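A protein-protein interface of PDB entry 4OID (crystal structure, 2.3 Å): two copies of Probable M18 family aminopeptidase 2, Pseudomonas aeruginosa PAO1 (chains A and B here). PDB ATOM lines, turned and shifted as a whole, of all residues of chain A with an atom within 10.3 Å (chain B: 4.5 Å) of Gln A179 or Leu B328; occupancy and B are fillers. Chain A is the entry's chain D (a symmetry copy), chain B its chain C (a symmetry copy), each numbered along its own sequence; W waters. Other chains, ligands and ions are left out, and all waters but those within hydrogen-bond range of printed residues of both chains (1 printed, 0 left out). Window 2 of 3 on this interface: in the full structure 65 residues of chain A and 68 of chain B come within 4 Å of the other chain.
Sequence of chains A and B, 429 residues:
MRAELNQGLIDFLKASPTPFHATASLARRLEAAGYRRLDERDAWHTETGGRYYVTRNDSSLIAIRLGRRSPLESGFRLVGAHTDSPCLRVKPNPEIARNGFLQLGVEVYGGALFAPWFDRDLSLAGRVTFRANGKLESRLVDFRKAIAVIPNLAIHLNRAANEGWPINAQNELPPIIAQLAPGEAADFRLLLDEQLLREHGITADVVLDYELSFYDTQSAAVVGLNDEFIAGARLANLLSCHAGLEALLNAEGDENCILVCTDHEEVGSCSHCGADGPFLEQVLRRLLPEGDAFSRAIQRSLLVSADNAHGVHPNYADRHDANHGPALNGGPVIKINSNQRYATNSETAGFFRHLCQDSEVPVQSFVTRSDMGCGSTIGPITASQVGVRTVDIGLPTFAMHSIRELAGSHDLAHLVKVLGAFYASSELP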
ATOM      1  N   ILE A  96     -15.904 -21.151  -4.224  1.00  0.00           N
ATOM      2  CA  ILE A  96     -16.047 -20.127  -3.184  1.00  0.00           C
ATOM      3  C   ILE A  96     -14.916 -19.120  -3.408  1.00  0.00           C
ATOM      4  O   ILE A  96     -13.721 -19.498  -3.359  1.00  0.00           O
ATOM      5  CB  ILE A  96     -15.912 -20.725  -1.763  1.00  0.00           C
ATOM      6  CG1 ILE A  96     -17.156 -21.592  -1.406  1.00  0.00           C
ATOM      7  CG2 ILE A  96     -15.756 -19.609  -0.711  1.00  0.00           C
ATOM      8  CD1 ILE A  96     -17.120 -22.250  -0.039  1.00  0.00           C
ATOM      9  N   ALA A  97     -15.239 -17.871  -3.718  1.00  0.00           N
ATOM     10  CA  ALA A  97     -14.147 -16.903  -4.054  1.00  0.00           C
ATOM     11  C   ALA A  97     -14.177 -15.842  -3.010  1.00  0.00           C
ATOM     12  O   ALA A  97     -15.100 -15.065  -3.021  1.00  0.00           O
ATOM     13  CB  ALA A  97     -14.295 -16.299  -5.457  1.00  0.00           C
ATOM     14  N   ARG A  98     -13.215 -15.871  -2.074  1.00  0.00           N
ATOM     15  CA  ARG A  98     -13.150 -14.960  -0.915  1.00  0.00           C
ATOM     16  C   ARG A  98     -11.720 -14.501  -0.604  1.00  0.00           C
ATOM     17  O   ARG A  98     -10.795 -15.334  -0.582  1.00  0.00           O
ATOM     18  CB  ARG A  98     -13.741 -15.621   0.313  1.00  0.00           C
ATOM     19  CG  ARG A  98     -15.251 -15.490   0.360  1.00  0.00           C
ATOM     20  CD  ARG A  98     -15.891 -15.974   1.639  1.00  0.00           C
ATOM     21  NE  ARG A  98     -15.166 -17.155   2.124  1.00  0.00           N
ATOM     22  CZ  ARG A  98     -15.725 -18.191   2.745  1.00  0.00           C
ATOM     23  NH1 ARG A  98     -17.049 -18.234   2.944  1.00  0.00           N
ATOM     24  NH2 ARG A  98     -14.949 -19.203   3.144  1.00  0.00           N
ATOM     25  N   ASN A  99     -11.548 -13.183  -0.387  1.00  0.00           N
ATOM     26  CA  ASN A  99     -10.269 -12.561  -0.073  1.00  0.00           C
ATOM     27  C   ASN A  99      -9.153 -12.986  -0.990  1.00  0.00           C
ATOM     28  O   ASN A  99      -8.062 -13.374  -0.537  1.00  0.00           O
ATOM     29  CB  ASN A  99      -9.804 -12.930   1.349  1.00  0.00           C
ATOM     30  CG  ASN A  99     -10.805 -12.563   2.430  1.00  0.00           C
ATOM     31  OD1 ASN A  99     -11.509 -13.395   2.901  1.00  0.00           O
ATOM     32  ND2 ASN A  99     -10.801 -11.330   2.861  1.00  0.00           N
ATOM     33  N   GLY A 100      -9.399 -12.984  -2.279  1.00  0.00           N
ATOM     34  CA  GLY A 100      -8.334 -13.375  -3.233  1.00  0.00           C
ATOM     35  C   GLY A 100      -8.121 -14.886  -3.412  1.00  0.00           C
ATOM     36  O   GLY A 100      -7.350 -15.301  -4.326  1.00  0.00           O
ATOM     37  N   PHE A 101      -8.769 -15.720  -2.588  1.00  0.00           N
ATOM     38  CA  PHE A 101      -8.630 -17.164  -2.733  1.00  0.00           C
ATOM     39  C   PHE A 101      -9.729 -17.853  -3.520  1.00  0.00           C
ATOM     40  O   PHE A 101     -10.873 -17.406  -3.535  1.00  0.00           O
ATOM     41  CB  PHE A 101      -8.561 -17.870  -1.375  1.00  0.00           C
ATOM     42  CG  PHE A 101      -7.397 -17.449  -0.570  1.00  0.00           C
ATOM     43  CD1 PHE A 101      -6.170 -18.023  -0.771  1.00  0.00           C
ATOM     44  CD2 PHE A 101      -7.520 -16.463   0.340  1.00  0.00           C
ATOM     45  CE1 PHE A 101      -5.079 -17.634  -0.012  1.00  0.00           C
ATOM     46  CE2 PHE A 101      -6.436 -16.040   1.069  1.00  0.00           C
ATOM     47  CZ  PHE A 101      -5.224 -16.647   0.920  1.00  0.00           C
ATOM     48  N   LEU A 102      -9.375 -18.987  -4.131  1.00  0.00           N
ATOM     49  CA  LEU A 102     -10.382 -19.967  -4.533  1.00  0.00           C
ATOM     50  C   LEU A 102     -10.427 -21.146  -3.563  1.00  0.00           C
ATOM     51  O   LEU A 102      -9.407 -21.840  -3.322  1.00  0.00           O
ATOM     52  CB  LEU A 102     -10.138 -20.419  -5.941  1.00  0.00           C
ATOM     53  CG  LEU A 102     -11.132 -21.456  -6.499  1.00  0.00           C
ATOM     54  CD1 LEU A 102     -12.560 -20.873  -6.582  1.00  0.00           C
ATOM     55  CD2 LEU A 102     -10.574 -21.837  -7.874  1.00  0.00           C
ATOM     56  N   GLN A 103     -11.610 -21.351  -3.004  1.00  0.00           N
ATOM     57  CA  GLN A 103     -11.893 -22.464  -2.124  1.00  0.00           C
ATOM     58  C   GLN A 103     -13.008 -23.374  -2.715  1.00  0.00           C
ATOM     59  O   GLN A 103     -13.732 -22.969  -3.633  1.00  0.00           O
ATOM     60  CB  GLN A 103     -12.277 -21.995  -0.734  1.00  0.00           C
ATOM     61  CG  GLN A 103     -11.256 -21.201   0.024  1.00  0.00           C
ATOM     62  CD  GLN A 103     -11.846 -20.668   1.334  1.00  0.00           C
ATOM     63  OE1 GLN A 103     -12.425 -19.584   1.339  1.00  0.00           O
ATOM     64  NE2 GLN A 103     -11.788 -21.465   2.418  1.00  0.00           N
ATOM     65  N   ILE A 147      -2.762 -29.968  -3.873  1.00  0.00           N
ATOM     66  CA  ILE A 147      -3.382 -28.771  -4.438  1.00  0.00           C
ATOM     67  C   ILE A 147      -4.268 -28.046  -3.437  1.00  0.00           C
ATOM     68  O   ILE A 147      -4.820 -27.045  -3.793  1.00  0.00           O
ATOM     69  CB  ILE A 147      -4.263 -29.063  -5.668  1.00  0.00           C
ATOM     70  CG1 ILE A 147      -5.448 -29.962  -5.327  1.00  0.00           C
ATOM     71  CG2 ILE A 147      -3.535 -29.787  -6.783  1.00  0.00           C
ATOM     72  CD1 ILE A 147      -6.222 -30.268  -6.569  1.00  0.00           C
ATOM     73  N   ALA A 148      -4.366 -28.518  -2.198  1.00  0.00           N
ATOM     74  CA  ALA A 148      -5.352 -28.030  -1.272  1.00  0.00           C
ATOM     75  C   ALA A 148      -4.818 -28.088   0.143  1.00  0.00           C
ATOM     76  O   ALA A 148      -4.135 -29.041   0.541  1.00  0.00           O
ATOM     77  CB  ALA A 148      -6.635 -28.883  -1.346  1.00  0.00           C
ATOM     78  N   VAL A 149      -5.263 -27.144   0.943  1.00  0.00           N
ATOM     79  CA  VAL A 149      -4.931 -27.106   2.373  1.00  0.00           C
ATOM     80  C   VAL A 149      -6.068 -26.406   3.092  1.00  0.00           C
ATOM     81  O   VAL A 149      -6.715 -25.485   2.551  1.00  0.00           O
ATOM     82  CB  VAL A 149      -3.588 -26.369   2.585  1.00  0.00           C
ATOM     83  CG1 VAL A 149      -3.700 -25.015   1.899  1.00  0.00           C
ATOM     84  CG2 VAL A 149      -3.270 -26.190   4.070  1.00  0.00           C
ATOM     85  N   PRO A 151      -6.088 -24.531   6.308  1.00  0.00           N
ATOM     86  CA  PRO A 151      -5.189 -24.054   7.369  1.00  0.00           C
ATOM     87  C   PRO A 151      -5.912 -23.816   8.646  1.00  0.00           C
ATOM     88  O   PRO A 151      -7.004 -23.263   8.608  1.00  0.00           O
ATOM     89  CB  PRO A 151      -4.691 -22.685   6.844  1.00  0.00           C
ATOM     90  CG  PRO A 151      -5.244 -22.575   5.448  1.00  0.00           C
ATOM     91  CD  PRO A 151      -6.434 -23.466   5.359  1.00  0.00           C
ATOM     92  N   ASN A 152      -5.283 -24.172   9.770  1.00  0.00           N
ATOM     93  CA  ASN A 152      -5.746 -23.665  11.058  1.00  0.00           C
ATOM     94  C   ASN A 152      -5.692 -22.125  11.141  1.00  0.00           C
ATOM     95  O   ASN A 152      -4.894 -21.460  10.434  1.00  0.00           O
ATOM     96  CB  ASN A 152      -4.901 -24.207  12.236  1.00  0.00           C
ATOM     97  CG  ASN A 152      -5.502 -25.459  12.862  1.00  0.00           C
ATOM     98  OD1 ASN A 152      -6.638 -25.424  13.331  1.00  0.00           O
ATOM     99  ND2 ASN A 152      -4.728 -26.548  12.915  1.00  0.00           N
ATOM    100  N   PRO A 175     -11.393 -26.220   1.694  1.00  0.00           N
ATOM    101  CA  PRO A 175      -9.974 -26.040   1.448  1.00  0.00           C
ATOM    102  C   PRO A 175      -9.665 -24.958   0.499  1.00  0.00           C
ATOM    103  O   PRO A 175     -10.471 -24.705  -0.415  1.00  0.00           O
ATOM    104  CB  PRO A 175      -9.534 -27.346   0.873  1.00  0.00           C
ATOM    105  CG  PRO A 175     -10.659 -28.299   1.154  1.00  0.00           C
ATOM    106  CD  PRO A 175     -11.896 -27.524   1.269  1.00  0.00           C
ATOM    107  N   ILE A 176      -8.490 -24.334   0.690  1.00  0.00           N
ATOM    108  CA  ILE A 176      -7.966 -23.374  -0.266  1.00  0.00           C
ATOM    109  C   ILE A 176      -7.240 -24.149  -1.353  1.00  0.00           C
ATOM    110  O   ILE A 176      -6.418 -24.989  -1.050  1.00  0.00           O
ATOM    111  CB  ILE A 176      -6.938 -22.405   0.376  1.00  0.00           C
ATOM    112  CG1 ILE A 176      -7.598 -21.505   1.411  1.00  0.00           C
ATOM    113  CG2 ILE A 176      -6.199 -21.581  -0.686  1.00  0.00           C
ATOM    114  CD1 ILE A 176      -6.652 -20.895   2.448  1.00  0.00           C
ATOM    115  N   ILE A 177      -7.509 -23.851  -2.615  1.00  0.00           N
ATOM    116  CA  ILE A 177      -6.741 -24.479  -3.726  1.00  0.00           C
ATOM    117  C   ILE A 177      -5.914 -23.501  -4.609  1.00  0.00           C
ATOM    118  O   ILE A 177      -4.954 -23.898  -5.236  1.00  0.00           O
ATOM    119  CB  ILE A 177      -7.647 -25.332  -4.623  1.00  0.00           C
ATOM    120  CG1 ILE A 177      -8.636 -24.471  -5.396  1.00  0.00           C
ATOM    121  CG2 ILE A 177      -8.452 -26.350  -3.805  1.00  0.00           C
ATOM    122  CD1 ILE A 177      -9.260 -25.249  -6.573  1.00  0.00           C
ATOM    123  N   ALA A 178      -6.274 -22.225  -4.642  1.00  0.00           N
ATOM    124  CA  ALA A 178      -5.616 -21.275  -5.502  1.00  0.00           C
ATOM    125  C   ALA A 178      -5.829 -19.860  -5.006  1.00  0.00           C
ATOM    126  O   ALA A 178      -6.609 -19.628  -4.108  1.00  0.00           O
ATOM    127  CB  ALA A 178      -6.089 -21.438  -6.944  1.00  0.00           C
ATOM    128  N   GLN A 179      -5.096 -18.926  -5.595  1.00  0.00           N
ATOM    129  CA  GLN A 179      -5.445 -17.504  -5.594  1.00  0.00           C
ATOM    130  C   GLN A 179      -5.910 -17.118  -7.009  1.00  0.00           C
ATOM    131  O   GLN A 179      -5.429 -17.637  -7.991  1.00  0.00           O
ATOM    132  CB  GLN A 179      -4.221 -16.651  -5.214  1.00  0.00           C
ATOM    133  CG  GLN A 179      -3.905 -16.784  -3.742  1.00  0.00           C
ATOM    134  CD  GLN A 179      -2.648 -16.095  -3.352  1.00  0.00           C
ATOM    135  OE1 GLN A 179      -1.568 -16.410  -3.851  1.00  0.00           O
ATOM    136  NE2 GLN A 179      -2.776 -15.132  -2.504  1.00  0.00           N
ATOM    137  N   LEU A 180      -6.795 -16.155  -7.093  1.00  0.00           N
ATOM    138  CA  LEU A 180      -7.405 -15.785  -8.351  1.00  0.00           C
ATOM    139  C   LEU A 180      -6.923 -14.403  -8.740  1.00  0.00           C
ATOM    140  O   LEU A 180      -6.951 -13.523  -7.897  1.00  0.00           O
ATOM    141  CB  LEU A 180      -8.938 -15.702  -8.112  1.00  0.00           C
ATOM    142  CG  LEU A 180      -9.749 -16.975  -7.851  1.00  0.00           C
ATOM    143  CD1 LEU A 180     -11.130 -16.636  -7.315  1.00  0.00           C
ATOM    144  CD2 LEU A 180      -9.889 -17.742  -9.111  1.00  0.00           C
ATOM    145  N   ALA A 181      -6.555 -14.186  -9.999  1.00  0.00           N
ATOM    146  CA  ALA A 181      -6.243 -12.808 -10.522  1.00  0.00           C
ATOM    147  C   ALA A 181      -7.516 -11.929 -10.365  1.00  0.00           C
ATOM    148  O   ALA A 181      -8.646 -12.442 -10.353  1.00  0.00           O
ATOM    149  N   PRO A 182      -7.353 -10.612 -10.234  1.00  0.00           N
ATOM    150  CA  PRO A 182      -8.552  -9.766 -10.102  1.00  0.00           C
ATOM    151  C   PRO A 182      -9.443  -9.840 -11.361  1.00  0.00           C
ATOM    152  O   PRO A 182      -8.934  -9.773 -12.477  1.00  0.00           O
ATOM    153  CB  PRO A 182      -7.964  -8.365  -9.891  1.00  0.00           C
ATOM    154  CG  PRO A 182      -6.624  -8.397 -10.562  1.00  0.00           C
ATOM    155  CD  PRO A 182      -6.144  -9.830 -10.562  1.00  0.00           C
ATOM    156  N   GLY A 183     -10.742 -10.057 -11.185  1.00  0.00           N
ATOM    157  CA  GLY A 183     -11.646 -10.364 -12.319  1.00  0.00           C
ATOM    158  C   GLY A 183     -11.549 -11.732 -13.021  1.00  0.00           C
ATOM    159  O   GLY A 183     -12.029 -11.886 -14.129  1.00  0.00           O
ATOM    160  N   GLU A 184     -10.945 -12.737 -12.397  1.00  0.00           N
ATOM    161  CA  GLU A 184     -10.825 -14.064 -13.014  1.00  0.00           C
ATOM    162  C   GLU A 184     -11.993 -14.914 -12.552  1.00  0.00           C
ATOM    163  O   GLU A 184     -12.356 -14.918 -11.376  1.00  0.00           O
ATOM    164  CB  GLU A 184      -9.469 -14.687 -12.650  1.00  0.00           C
ATOM    165  CG  GLU A 184      -9.248 -16.157 -12.981  1.00  0.00           C
ATOM    166  CD  GLU A 184      -7.846 -16.627 -12.579  1.00  0.00           C
ATOM    167  OE1 GLU A 184      -7.179 -15.915 -11.808  1.00  0.00           O
ATOM    168  OE2 GLU A 184      -7.398 -17.718 -13.022  1.00  0.00           O
ATOM    169  N   ALA A 185     -12.632 -15.576 -13.498  1.00  0.00           N
ATOM    170  CA  ALA A 185     -13.719 -16.483 -13.188  1.00  0.00           C
ATOM    171  C   ALA A 185     -13.124 -17.803 -12.649  1.00  0.00           C
ATOM    172  O   ALA A 185     -12.003 -18.147 -12.965  1.00  0.00           O
ATOM    173  CB  ALA A 185     -14.552 -16.740 -14.425  1.00  0.00           C
ATOM    174  N   ALA A 186     -13.904 -18.488 -11.828  1.00  0.00           N
ATOM    175  CA  ALA A 186     -13.552 -19.729 -11.175  1.00  0.00           C
ATOM    176  C   ALA A 186     -14.508 -20.769 -11.741  1.00  0.00           C
ATOM    177  O   ALA A 186     -15.707 -20.629 -11.536  1.00  0.00           O
ATOM    178  CB  ALA A 186     -13.833 -19.585  -9.670  1.00  0.00           C
ATOM    179  N   GLU B 228       1.089 -21.856  -5.514  1.00  0.00           N
ATOM    180  CA  GLU B 228       1.105 -20.597  -4.820  1.00  0.00           C
ATOM    181  C   GLU B 228       1.603 -20.587  -3.363  1.00  0.00           C
ATOM    182  O   GLU B 228       1.729 -19.486  -2.760  1.00  0.00           O
ATOM    183  CB  GLU B 228      -0.299 -20.014  -4.744  1.00  0.00           C
ATOM    184  CG  GLU B 228      -0.985 -19.773  -6.061  1.00  0.00           C
ATOM    185  CD  GLU B 228      -1.983 -20.889  -6.434  1.00  0.00           C
ATOM    186  OE1 GLU B 228      -1.731 -22.151  -6.230  1.00  0.00           O
ATOM    187  OE2 GLU B 228      -3.016 -20.457  -6.967  1.00  0.00           O
ATOM    188  N   PHE B 229       1.758 -21.749  -2.751  1.00  0.00           N
ATOM    189  CA  PHE B 229       1.943 -21.774  -1.297  1.00  0.00           C
ATOM    190  C   PHE B 229       3.098 -22.630  -0.901  1.00  0.00           C
ATOM    191  O   PHE B 229       3.489 -23.481  -1.668  1.00  0.00           O
ATOM    192  CB  PHE B 229       0.688 -22.276  -0.553  1.00  0.00           C
ATOM    193  CG  PHE B 229      -0.565 -21.613  -0.976  1.00  0.00           C
ATOM    194  CD1 PHE B 229      -0.786 -20.251  -0.724  1.00  0.00           C
ATOM    195  CD2 PHE B 229      -1.532 -22.317  -1.689  1.00  0.00           C
ATOM    196  CE1 PHE B 229      -1.975 -19.630  -1.106  1.00  0.00           C
ATOM    197  CE2 PHE B 229      -2.710 -21.701  -2.098  1.00  0.00           C
ATOM    198  CZ  PHE B 229      -2.923 -20.342  -1.808  1.00  0.00           C
ATOM    199  N   GLY B 311      -1.831 -13.636   7.732  1.00  0.00           N
ATOM    200  CA  GLY B 311      -2.634 -13.365   6.535  1.00  0.00           C
ATOM    201  C   GLY B 311      -4.094 -13.339   6.966  1.00  0.00           C
ATOM    202  O   GLY B 311      -4.439 -14.051   7.902  1.00  0.00           O
ATOM    203  N   PRO B 326      -3.734  -8.741   5.376  1.00  0.00           N
ATOM    204  CA  PRO B 326      -2.669  -9.010   4.413  1.00  0.00           C
ATOM    205  C   PRO B 326      -2.866 -10.338   3.659  1.00  0.00           C
ATOM    206  O   PRO B 326      -3.313 -11.339   4.240  1.00  0.00           O
ATOM    207  CB  PRO B 326      -1.398  -9.024   5.270  1.00  0.00           C
ATOM    208  CG  PRO B 326      -1.841  -8.687   6.664  1.00  0.00           C
ATOM    209  CD  PRO B 326      -3.297  -9.041   6.746  1.00  0.00           C
ATOM    210  N   ALA B 327      -2.562 -10.289   2.366  1.00  0.00           N
ATOM    211  CA  ALA B 327      -2.604 -11.403   1.479  1.00  0.00           C
ATOM    212  C   ALA B 327      -1.249 -12.160   1.430  1.00  0.00           C
ATOM    213  O   ALA B 327      -0.181 -11.562   1.256  1.00  0.00           O
ATOM    214  CB  ALA B 327      -2.965 -10.926   0.037  1.00  0.00           C
ATOM    215  N   LEU B 328      -1.331 -13.476   1.494  1.00  0.00           N
ATOM    216  CA  LEU B 328      -0.279 -14.332   1.047  1.00  0.00           C
ATOM    217  C   LEU B 328       0.097 -13.948  -0.376  1.00  0.00           C
ATOM    218  O   LEU B 328      -0.774 -13.687  -1.177  1.00  0.00           O
ATOM    219  CB  LEU B 328      -0.741 -15.774   1.079  1.00  0.00           C
ATOM    220  CG  LEU B 328      -0.483 -16.510   2.361  1.00  0.00           C
ATOM    221  CD1 LEU B 328      -1.161 -15.788   3.502  1.00  0.00           C
ATOM    222  CD2 LEU B 328      -0.917 -17.974   2.208  1.00  0.00           C
ATOM    223  N   ASN B 329       1.394 -13.953  -0.669  1.00  0.00           N
ATOM    224  CA  ASN B 329       1.983 -13.496  -1.905  1.00  0.00           C
ATOM    225  C   ASN B 329       1.758 -12.010  -2.166  1.00  0.00           C
ATOM    226  O   ASN B 329       2.006 -11.540  -3.242  1.00  0.00           O
ATOM    227  CB  ASN B 329       1.511 -14.354  -3.072  1.00  0.00           C
ATOM    228  CG  ASN B 329       1.955 -15.792  -2.900  1.00  0.00           C
ATOM    229  OD1 ASN B 329       3.137 -16.047  -2.618  1.00  0.00           O
ATOM    230  ND2 ASN B 329       1.028 -16.733  -3.048  1.00  0.00           N
ATOM    231  N   GLY B 330       1.300 -11.266  -1.185  1.00  0.00           N
ATOM    232  CA  GLY B 330       1.070  -9.811  -1.350  1.00  0.00           C
ATOM    233  C   GLY B 330       2.255  -8.967  -0.871  1.00  0.00           C
ATOM    234  O   GLY B 330       2.165  -7.761  -0.876  1.00  0.00           O
ATOM    235  N   PRO B 396       3.303 -12.753   5.457  1.00  0.00           N
ATOM    236  CA  PRO B 396       1.980 -13.215   5.748  1.00  0.00           C
ATOM    237  C   PRO B 396       1.937 -14.755   5.775  1.00  0.00           C
ATOM    238  O   PRO B 396       2.436 -15.404   4.859  1.00  0.00           O
ATOM    239  CB  PRO B 396       1.155 -12.649   4.589  1.00  0.00           C
ATOM    240  CG  PRO B 396       2.142 -12.079   3.583  1.00  0.00           C
ATOM    241  CD  PRO B 396       3.510 -12.366   4.051  1.00  0.00           C
ATOM    242  N   THR B 397       1.240 -15.290   6.763  1.00  0.00           N
ATOM    243  CA  THR B 397       1.281 -16.679   7.135  1.00  0.00           C
ATOM    244  C   THR B 397      -0.075 -17.114   7.697  1.00  0.00           C
ATOM    245  O   THR B 397      -0.770 -16.300   8.339  1.00  0.00           O
ATOM    246  CB  THR B 397       2.359 -16.745   8.234  1.00  0.00           C
ATOM    247  OG1 THR B 397       3.619 -17.087   7.630  1.00  0.00           O
ATOM    248  CG2 THR B 397       2.042 -17.670   9.263  1.00  0.00           C
ATOM    249  N   PHE B 398      -0.492 -18.350   7.434  1.00  0.00           N
ATOM    250  CA  PHE B 398      -1.647 -18.923   8.119  1.00  0.00           C
ATOM    251  C   PHE B 398      -1.212 -20.002   9.061  1.00  0.00           C
ATOM    252  O   PHE B 398      -0.194 -20.647   8.862  1.00  0.00           O
ATOM    253  CB  PHE B 398      -2.650 -19.566   7.176  1.00  0.00           C
ATOM    254  CG  PHE B 398      -3.368 -18.626   6.241  1.00  0.00           C
ATOM    255  CD1 PHE B 398      -3.643 -17.354   6.576  1.00  0.00           C
ATOM    256  CD2 PHE B 398      -3.733 -19.069   4.968  1.00  0.00           C
ATOM    257  CE1 PHE B 398      -4.313 -16.504   5.705  1.00  0.00           C
ATOM    258  CE2 PHE B 398      -4.351 -18.245   4.071  1.00  0.00           C
ATOM    259  CZ  PHE B 398      -4.667 -16.952   4.438  1.00  0.00           C
ATOM    260  N   LEU B 406       1.467 -22.248   6.781  1.00  0.00           N
ATOM    261  CA  LEU B 406       1.331 -21.998   5.323  1.00  0.00           C
ATOM    262  C   LEU B 406       1.759 -20.564   4.987  1.00  0.00           C
ATOM    263  O   LEU B 406       1.278 -19.628   5.600  1.00  0.00           O
ATOM    264  CB  LEU B 406      -0.113 -22.206   4.874  1.00  0.00           C
ATOM    265  CG  LEU B 406      -0.440 -22.269   3.376  1.00  0.00           C
ATOM    266  CD1 LEU B 406       0.049 -23.598   2.802  1.00  0.00           C
ATOM    267  CD2 LEU B 406      -1.920 -22.103   3.154  1.00  0.00           C
ATOM    268  N   ALA B 407       2.624 -20.415   3.985  1.00  0.00           N
ATOM    269  CA  ALA B 407       3.023 -19.126   3.520  1.00  0.00           C
ATOM    270  C   ALA B 407       2.926 -19.114   1.999  1.00  0.00           C
ATOM    271  O   ALA B 407       2.628 -20.120   1.328  1.00  0.00           O
ATOM    272  CB  ALA B 407       4.457 -18.818   3.997  1.00  0.00           C
ATOM    273  N   GLY B 408       3.178 -17.940   1.460  1.00  0.00           N
ATOM    274  CA  GLY B 408       3.114 -17.717   0.011  1.00  0.00           C
ATOM    275  C   GLY B 408       4.402 -18.168  -0.656  1.00  0.00           C
ATOM    276  O   GLY B 408       5.455 -17.954  -0.135  1.00  0.00           O
ATOM    277  N   ASP B 411       6.600 -15.066  -1.651  1.00  0.00           N
ATOM    278  CA  ASP B 411       6.983 -14.128  -0.614  1.00  0.00           C
ATOM    279  C   ASP B 411       8.437 -14.185  -0.184  1.00  0.00           C
ATOM    280  O   ASP B 411       9.004 -13.143   0.137  1.00  0.00           O
ATOM    281  CB  ASP B 411       6.023 -14.224   0.582  1.00  0.00           C
ATOM    282  CG  ASP B 411       4.657 -13.455   0.329  1.00  0.00           C
ATOM    283  OD1 ASP B 411       4.621 -12.455  -0.473  1.00  0.00           O
ATOM    284  OD2 ASP B 411       3.616 -13.863   0.947  1.00  0.00           O
HETATM  285  O   HOH W   1      -2.473 -18.328  -8.316  1.00  0.00           O
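Printed residues of chain B within 4 Å of Phe A101: Phe B229 and Phe B398. Of the printed residues of chain B, Val A149 touches Leu B406. Of chain B, only Glu B228 (2.9 Å), Leu B328 (2.8 Å) and Asn B329 (2.7 Å) come within 4 Å of Gln A179. Gly A183 touches none of the printed residues of chain B. No residue of chain A comes within 4 Å of Gly B311. No residue of chain A comes within 4 Å of Ala B327. Of chain A, only Gln A179 (2.8 Å) comes within 4 Å of Leu B328. Of chain A, only Gln A179 comes within 4 Å of Asn B329. No residue of chain A comes within 4 Å of Pro B396. No residue of chain A comes within 4 Å of Ala B407. The nearest residue of chain B that does not touch Gln A179 is Phe B229 (4.2 Å). The nearest residue of chain A that does not touch Leu B328 is Phe A101 (4.6 Å). The nearest printed residue of chain B that does not touch Ile A177 is Phe B229 (4.4 Å).
No position is printed for both chains.
N of Ile A177 lies within hydrogen-bond range of O of Leu A102 (2.9 Å). ND2 of Asn B329 lies within hydrogen-bond range of O of Glu B228, at 2.9 Å. The backbone NH of Asn B329 sits at hydrogen-bond distance from the side-chain carboxylate of Asp B411. The backbone carbonyl oxygen (O) of Leu B406 sits at hydrogen-bond distance from the backbone NH (N) of Phe B398. The backbone carbonyl oxygen (O) of Val A149 is in hydrogen-bond range of the backbone NH (N) of Ile A176. The backbone NH (N) of Leu A102 is in hydrogen-bond range of the backbone carbonyl oxygen (O) of Ala A178 (2.8 Å).
Water W1 lies within hydrogen-bond range of OE2 of Glu B228 (2.6 Å) and O of Gln A179 (3.1 Å).
Of the 15 printed residues of chain B, 6 touch a printed residue of chain A. Of the 25 printed residues of chain A, 7 touch a printed residue of chain B. Hydrophobic or aromatic side chains of chain A that line the printed part of chain B: Phe A101, Val A149, Pro A151, Ile A176 and Ala A178. Among the printed residues, 11 pairs touch across the chains.
Among the printed residues, pairs that only touch across the chains: Ala A178 with Glu B228 (3.1 Å), Phe A101 with Phe B398 (3.6 Å), Val A149 with Leu B406 (3.6 Å), Ile A176 with Phe B229 (3.7 Å), Pro A151 with Phe B398 (3.7 Å), Ile A177 with Glu B228 (3.8 Å), Phe A101 with Phe B229 (3.8 Å) and Ile A176 with Phe B398 (3.9 Å).
The side-chain amide nitrogen (ND2) of Asn B329 lies within hydrogen-bond range of the side-chain amide oxygen (OE1) of Gln A179 (2.7 Å). The backbone NH (N) of Gln A179 lies within hydrogen-bond range of the side-chain carboxylate (OE2) of Glu B228. The backbone carbonyl oxygen of Leu B328 is in hydrogen-bond range of the side-chain amide nitrogen of Gln A179 (2.8 Å).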
